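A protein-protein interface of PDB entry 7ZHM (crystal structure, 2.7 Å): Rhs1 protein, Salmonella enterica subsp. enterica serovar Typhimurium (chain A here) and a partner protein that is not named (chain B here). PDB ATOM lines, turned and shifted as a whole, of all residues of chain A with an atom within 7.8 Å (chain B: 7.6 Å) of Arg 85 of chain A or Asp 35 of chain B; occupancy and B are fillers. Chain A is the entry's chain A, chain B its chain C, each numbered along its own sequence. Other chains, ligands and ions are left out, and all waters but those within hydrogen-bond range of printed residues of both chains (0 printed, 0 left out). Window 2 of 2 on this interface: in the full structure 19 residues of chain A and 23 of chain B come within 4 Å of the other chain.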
ATOM      1  N   GLU A  79     -25.298   6.566  28.337  1.00  0.00           N
ATOM      2  CA  GLU A  79     -26.718   6.569  28.703  1.00  0.00           C
ATOM      3  C   GLU A  79     -27.513   7.548  27.820  1.00  0.00           C
ATOM      4  O   GLU A  79     -28.647   7.266  27.434  1.00  0.00           O
ATOM      5  CB  GLU A  79     -26.888   6.927  30.188  1.00  0.00           C
ATOM      6  CG  GLU A  79     -28.073   6.273  30.886  1.00  0.00           C
ATOM      7  CD  GLU A  79     -27.820   4.816  31.257  1.00  0.00           C
ATOM      8  OE1 GLU A  79     -26.906   4.537  32.073  1.00  0.00           O
ATOM      9  OE2 GLU A  79     -28.557   3.945  30.747  1.00  0.00           O
ATOM     10  N   GLY A  80     -26.896   8.690  27.498  1.00  0.00           N
ATOM     11  CA  GLY A  80     -27.484   9.701  26.634  1.00  0.00           C
ATOM     12  C   GLY A  80     -27.645   9.267  25.184  1.00  0.00           C
ATOM     13  O   GLY A  80     -28.648   9.586  24.543  1.00  0.00           O
ATOM     14  N   ARG A  81     -26.644   8.543  24.669  1.00  0.00           N
ATOM     15  CA  ARG A  81     -26.630   7.997  23.282  1.00  0.00           C
ATOM     16  C   ARG A  81     -27.645   6.853  23.164  1.00  0.00           C
ATOM     17  O   ARG A  81     -28.231   6.700  22.073  1.00  0.00           O
ATOM     18  CB  ARG A  81     -25.223   7.531  22.893  1.00  0.00           C
ATOM     19  CG  ARG A  81     -24.236   8.663  22.647  1.00  0.00           C
ATOM     20  CD  ARG A  81     -24.568   9.491  21.419  1.00  0.00           C
ATOM     21  NE  ARG A  81     -23.579  10.537  21.198  1.00  0.00           N
ATOM     22  CZ  ARG A  81     -22.373  10.356  20.664  1.00  0.00           C
ATOM     23  NH1 ARG A  81     -21.975   9.154  20.279  1.00  0.00           N
ATOM     24  NH2 ARG A  81     -21.560  11.388  20.518  1.00  0.00           N
ATOM     25  N   LEU A  82     -27.837   6.084  24.242  1.00  0.00           N
ATOM     26  CA  LEU A  82     -28.859   5.042  24.299  1.00  0.00           C
ATOM     27  C   LEU A  82     -30.236   5.669  24.141  1.00  0.00           C
ATOM     28  O   LEU A  82     -31.011   5.266  23.276  1.00  0.00           O
ATOM     29  CB  LEU A  82     -28.782   4.272  25.623  1.00  0.00           C
ATOM     30  CG  LEU A  82     -29.733   3.081  25.786  1.00  0.00           C
ATOM     31  CD1 LEU A  82     -29.493   2.045  24.697  1.00  0.00           C
ATOM     32  CD2 LEU A  82     -29.577   2.455  27.163  1.00  0.00           C
ATOM     33  N   ALA A  83     -30.514   6.674  24.979  1.00  0.00           N
ATOM     34  CA  ALA A  83     -31.776   7.408  24.976  1.00  0.00           C
ATOM     35  C   ALA A  83     -32.137   7.942  23.590  1.00  0.00           C
ATOM     36  O   ALA A  83     -33.292   7.856  23.174  1.00  0.00           O
ATOM     37  CB  ALA A  83     -31.724   8.551  25.986  1.00  0.00           C
ATOM     38  N   LYS A  84     -31.143   8.497  22.885  1.00  0.00           N
ATOM     39  CA  LYS A  84     -31.328   9.014  21.528  1.00  0.00           C
ATOM     40  C   LYS A  84     -31.795   7.911  20.596  1.00  0.00           C
ATOM     41  O   LYS A  84     -32.736   8.096  19.835  1.00  0.00           O
ATOM     42  CB  LYS A  84     -30.033   9.620  20.985  1.00  0.00           C
ATOM     43  CG  LYS A  84     -30.208  10.424  19.702  1.00  0.00           C
ATOM     44  CD  LYS A  84     -28.976  11.265  19.380  1.00  0.00           C
ATOM     45  CE  LYS A  84     -27.740  10.424  19.056  1.00  0.00           C
ATOM     46  NZ  LYS A  84     -27.854   9.688  17.762  1.00  0.00           N
ATOM     47  N   ARG A  85     -31.129   6.756  20.679  1.00  0.00           N
ATOM     48  CA  ARG A  85     -31.360   5.579  19.799  1.00  0.00           C
ATOM     49  C   ARG A  85     -32.739   4.970  20.084  1.00  0.00           C
ATOM     50  O   ARG A  85     -33.436   4.627  19.113  1.00  0.00           O
ATOM     51  CB  ARG A  85     -30.263   4.531  19.999  1.00  0.00           C
ATOM     52  CG  ARG A  85     -30.302   3.416  18.968  1.00  0.00           C
ATOM     53  CD  ARG A  85     -29.763   2.107  19.507  1.00  0.00           C
ATOM     54  NE  ARG A  85     -29.438   1.170  18.441  1.00  0.00           N
ATOM     55  CZ  ARG A  85     -28.300   1.162  17.751  1.00  0.00           C
ATOM     56  NH1 ARG A  85     -27.355   2.055  17.997  1.00  0.00           N
ATOM     57  NH2 ARG A  85     -28.114   0.259  16.805  1.00  0.00           N
ATOM     58  N   LYS A  86     -33.105   4.839  21.365  1.00  0.00           N
ATOM     59  CA  LYS A  86     -34.395   4.278  21.780  1.00  0.00           C
ATOM     60  C   LYS A  86     -35.590   5.218  21.566  1.00  0.00           C
ATOM     61  O   LYS A  86     -36.738   4.784  21.641  1.00  0.00           O
ATOM     62  CB  LYS A  86     -34.344   3.866  23.259  1.00  0.00           C
ATOM     63  CG  LYS A  86     -33.476   2.652  23.547  1.00  0.00           C
ATOM     64  CD  LYS A  86     -34.112   1.363  23.042  1.00  0.00           C
ATOM     65  CE  LYS A  86     -33.222   0.164  23.329  1.00  0.00           C
ATOM     66  NZ  LYS A  86     -33.592  -1.036  22.526  1.00  0.00           N
ATOM     67  N   GLY A  87     -35.315   6.501  21.309  1.00  0.00           N
ATOM     68  CA  GLY A  87     -36.340   7.509  21.114  1.00  0.00           C
ATOM     69  C   GLY A  87     -36.910   8.018  22.426  1.00  0.00           C
ATOM     70  O   GLY A  87     -38.069   8.415  22.487  1.00  0.00           O
ATOM     71  N   LEU A  88     -36.079   8.004  23.474  1.00  0.00           N
ATOM     72  CA  LEU A  88     -36.443   8.491  24.800  1.00  0.00           C
ATOM     73  C   LEU A  88     -35.937   9.922  24.974  1.00  0.00           C
ATOM     74  O   LEU A  88     -35.079  10.371  24.217  1.00  0.00           O
ATOM     75  CB  LEU A  88     -35.833   7.603  25.886  1.00  0.00           C
ATOM     76  CG  LEU A  88     -36.122   6.105  25.799  1.00  0.00           C
ATOM     77  CD1 LEU A  88     -35.429   5.381  26.945  1.00  0.00           C
ATOM     78  CD2 LEU A  88     -37.623   5.847  25.802  1.00  0.00           C
ATOM     79  N   VAL A  90     -33.623  12.719  25.801  1.00  0.00           N
ATOM     80  CA  VAL A  90     -32.169  12.782  25.952  1.00  0.00           C
ATOM     81  C   VAL A  90     -31.820  13.710  27.111  1.00  0.00           C
ATOM     82  O   VAL A  90     -32.151  14.895  27.072  1.00  0.00           O
ATOM     83  CB  VAL A  90     -31.482  13.302  24.671  1.00  0.00           C
ATOM     84  CG1 VAL A  90     -29.968  13.389  24.866  1.00  0.00           C
ATOM     85  CG2 VAL A  90     -31.827  12.409  23.487  1.00  0.00           C
ATOM     86  N   PHE B  32     -17.610   3.598  18.923  1.00  0.00           N
ATOM     87  CA  PHE B  32     -18.135   2.616  17.984  1.00  0.00           C
ATOM     88  C   PHE B  32     -19.595   2.320  18.312  1.00  0.00           C
ATOM     89  O   PHE B  32     -19.980   2.273  19.482  1.00  0.00           O
ATOM     90  CB  PHE B  32     -17.309   1.328  17.991  1.00  0.00           C
ATOM     91  CG  PHE B  32     -17.734   0.339  16.940  1.00  0.00           C
ATOM     92  CD1 PHE B  32     -17.427   0.558  15.602  1.00  0.00           C
ATOM     93  CD2 PHE B  32     -18.451  -0.806  17.283  1.00  0.00           C
ATOM     94  CE1 PHE B  32     -17.828  -0.339  14.624  1.00  0.00           C
ATOM     95  CE2 PHE B  32     -18.856  -1.704  16.308  1.00  0.00           C
ATOM     96  CZ  PHE B  32     -18.541  -1.473  14.977  1.00  0.00           C
ATOM     97  N   GLU B  33     -20.399   2.136  17.259  1.00  0.00           N
ATOM     98  CA  GLU B  33     -21.827   1.886  17.385  1.00  0.00           C
ATOM     99  C   GLU B  33     -22.304   1.011  16.225  1.00  0.00           C
ATOM    100  O   GLU B  33     -21.969   1.265  15.069  1.00  0.00           O
ATOM    101  CB  GLU B  33     -22.578   3.219  17.416  1.00  0.00           C
ATOM    102  CG  GLU B  33     -24.088   3.096  17.583  1.00  0.00           C
ATOM    103  CD  GLU B  33     -24.767   4.418  17.925  1.00  0.00           C
ATOM    104  OE1 GLU B  33     -24.083   5.464  17.920  1.00  0.00           O
ATOM    105  OE2 GLU B  33     -25.991   4.423  18.188  1.00  0.00           O
ATOM    106  N   ASP B  34     -23.077  -0.030  16.555  1.00  0.00           N
ATOM    107  CA  ASP B  34     -23.675  -0.929  15.570  1.00  0.00           C
ATOM    108  C   ASP B  34     -25.054  -1.414  16.055  1.00  0.00           C
ATOM    109  O   ASP B  34     -25.677  -0.771  16.901  1.00  0.00           O
ATOM    110  CB  ASP B  34     -22.710  -2.087  15.242  1.00  0.00           C
ATOM    111  CG  ASP B  34     -22.510  -3.061  16.405  1.00  0.00           C
ATOM    112  OD1 ASP B  34     -23.306  -3.052  17.373  1.00  0.00           O
ATOM    113  OD2 ASP B  34     -21.537  -3.849  16.347  1.00  0.00           O
ATOM    114  N   ASP B  35     -25.517  -2.547  15.517  1.00  0.00           N
ATOM    115  CA  ASP B  35     -26.856  -3.067  15.784  1.00  0.00           C
ATOM    116  C   ASP B  35     -27.113  -3.424  17.250  1.00  0.00           C
ATOM    117  O   ASP B  35     -28.214  -3.198  17.755  1.00  0.00           O
ATOM    118  CB  ASP B  35     -27.122  -4.286  14.901  1.00  0.00           C
ATOM    119  CG  ASP B  35     -27.052  -3.952  13.422  1.00  0.00           C
ATOM    120  OD1 ASP B  35     -27.871  -3.127  12.963  1.00  0.00           O
ATOM    121  OD2 ASP B  35     -26.175  -4.506  12.722  1.00  0.00           O
ATOM    122  N   ARG B  36     -26.097  -3.979  17.923  1.00  0.00           N
ATOM    123  CA  ARG B  36     -26.249  -4.618  19.261  1.00  0.00           C
ATOM    124  C   ARG B  36     -25.561  -3.796  20.358  1.00  0.00           C
ATOM    125  O   ARG B  36     -26.065  -3.853  21.498  1.00  0.00           O
ATOM    126  CB  ARG B  36     -25.733  -6.062  19.246  1.00  0.00           C
ATOM    127  CG  ARG B  36     -24.318  -6.228  18.722  1.00  0.00           C
ATOM    128  CD  ARG B  36     -24.118  -7.545  17.994  1.00  0.00           C
ATOM    129  NE  ARG B  36     -22.730  -7.983  18.074  1.00  0.00           N
ATOM    130  CZ  ARG B  36     -21.702  -7.400  17.458  1.00  0.00           C
ATOM    131  NH1 ARG B  36     -21.884  -6.341  16.686  1.00  0.00           N
ATOM    132  NH2 ARG B  36     -20.483  -7.890  17.610  1.00  0.00           N
ATOM    133  N   TYR B  37     -24.490  -3.056  20.043  1.00  0.00           N
ATOM    134  CA  TYR B  37     -23.647  -2.342  21.042  1.00  0.00           C
ATOM    135  C   TYR B  37     -23.500  -0.850  20.706  1.00  0.00           C
ATOM    136  O   TYR B  37     -23.347  -0.493  19.521  1.00  0.00           O
ATOM    137  CB  TYR B  37     -22.268  -3.001  21.147  1.00  0.00           C
ATOM    138  CG  TYR B  37     -22.292  -4.429  21.628  1.00  0.00           C
ATOM    139  CD1 TYR B  37     -22.997  -4.794  22.766  1.00  0.00           C
ATOM    140  CD2 TYR B  37     -21.600  -5.421  20.951  1.00  0.00           C
ATOM    141  CE1 TYR B  37     -23.026  -6.107  23.210  1.00  0.00           C
ATOM    142  CE2 TYR B  37     -21.616  -6.739  21.383  1.00  0.00           C
ATOM    143  CZ  TYR B  37     -22.330  -7.082  22.518  1.00  0.00           C
ATOM    144  OH  TYR B  37     -22.359  -8.374  22.951  1.00  0.00           O
ATOM    145  N   ILE B  38     -23.542  -0.011  21.749  1.00  0.00           N
ATOM    146  CA  ILE B  38     -23.088   1.377  21.724  1.00  0.00           C
ATOM    147  C   ILE B  38     -21.916   1.451  22.696  1.00  0.00           C
ATOM    148  O   ILE B  38     -22.087   1.218  23.886  1.00  0.00           O
ATOM    149  CB  ILE B  38     -24.187   2.352  22.185  1.00  0.00           C
ATOM    150  CG1 ILE B  38     -25.306   2.415  21.144  1.00  0.00           C
ATOM    151  CG2 ILE B  38     -23.605   3.744  22.423  1.00  0.00           C
ATOM    152  CD1 ILE B  38     -26.577   3.062  21.646  1.00  0.00           C
ATOM    153  N   ASP B  55     -25.160  -2.735  25.972  1.00  0.00           N
ATOM    154  CA  ASP B  55     -26.028  -3.601  25.189  1.00  0.00           C
ATOM    155  C   ASP B  55     -27.354  -2.874  24.942  1.00  0.00           C
ATOM    156  O   ASP B  55     -28.081  -2.556  25.885  1.00  0.00           O
ATOM    157  CB  ASP B  55     -26.249  -4.923  25.931  1.00  0.00           C
ATOM    158  CG  ASP B  55     -27.115  -5.900  25.156  1.00  0.00           C
ATOM    159  OD1 ASP B  55     -28.250  -5.538  24.794  1.00  0.00           O
ATOM    160  OD2 ASP B  55     -26.655  -7.037  24.922  1.00  0.00           O
ATOM    161  N   VAL B  56     -27.658  -2.634  23.662  1.00  0.00           N
ATOM    162  CA  VAL B  56     -28.835  -1.880  23.235  1.00  0.00           C
ATOM    163  C   VAL B  56     -30.158  -2.555  23.616  1.00  0.00           C
ATOM    164  O   VAL B  56     -31.093  -1.884  24.052  1.00  0.00           O
ATOM    165  CB  VAL B  56     -28.789  -1.623  21.712  1.00  0.00           C
ATOM    166  CG1 VAL B  56     -30.082  -0.994  21.215  1.00  0.00           C
ATOM    167  CG2 VAL B  56     -27.595  -0.737  21.371  1.00  0.00           C
ATOM    168  N   ASP B  57     -30.224  -3.881  23.447  1.00  0.00           N
ATOM    169  CA  ASP B  57     -31.445  -4.658  23.690  1.00  0.00           C
ATOM    170  C   ASP B  57     -31.905  -4.611  25.148  1.00  0.00           C
ATOM    171  O   ASP B  57     -33.083  -4.416  25.420  1.00  0.00           O
ATOM    172  CB  ASP B  57     -31.256  -6.122  23.265  1.00  0.00           C
ATOM    173  CG  ASP B  57     -31.073  -6.286  21.764  1.00  0.00           C
ATOM    174  OD1 ASP B  57     -31.504  -5.397  20.995  1.00  0.00           O
ATOM    175  OD2 ASP B  57     -30.499  -7.319  21.352  1.00  0.00           O
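The backbone carbonyl oxygen (O) of Val 56 of chain B sits close to the side-chain amino group (NZ) of Lys 86 of chain A, 3.0 Å away.
O of Asp 34 of chain B is in hydrogen-bond range of NH2 of Arg 85 of chain A, at 2.6 Å.
NH1 of Arg 85 of chain A lies within salt-bridge range of OE2 of Glu 33 of chain B, 2.7 Å away.
The backbone carbonyl oxygen (O) of Arg 36 of chain B is in hydrogen-bond range of the backbone NH (N) of Val 56 of chain B, 3.0 Å away.
OD1 of Asp 34 of chain B lies within hydrogen-bond range of N of Tyr 37 of chain B, 2.9 Å away.
The side-chain carboxylate of Asp 34 of chain B is in salt-bridge range of the guanidinium group of Arg 36 of chain B, at 2.5 Å.
Arg 85 of chain A touches Asp 35 of chain B.
Ile 38 of chain B touches Arg 85 of chain A.
Val 56 of chain B touches Arg 85 of chain A (CG1 to CD, 3.6 Å).
Ala 83 of chain A touches none of the printed residues of chain B.
Arg 85 of chain A touches just these residues of chain B: Glu 33 (2.7 Å), Asp 34 (2.6 Å), Asp 35 (3.6 Å), Ile 38 (3.8 Å) and Val 56 (3.6 Å).
Printed residues of chain A within 4 Å of Glu 33 of chain B: Arg 85 (2.7 Å).
Printed residues of chain A within 4 Å of Asp 34 of chain B: Arg 85 (2.6 Å).
Asp 35 of chain B touches one residue of chain A.
Of the printed residues of chain A, Val 56 of chain B touches Arg 85 and Lys 86.
Hydrophobic or aromatic side chains of chain B that line the printed part of chain A: Ile 38 and Val 56.
Printed residues of chain A that touch a printed residue of chain B: Arg 85 and Lys 86.
Among the printed residues, 6 pairs touch across the chains.
Among the printed residues, Asp or Glu carboxylates within 4 Å of a Lys or Arg side-chain nitrogen of the other chain: Arg 85 of chain A with Glu 33 of chain B.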
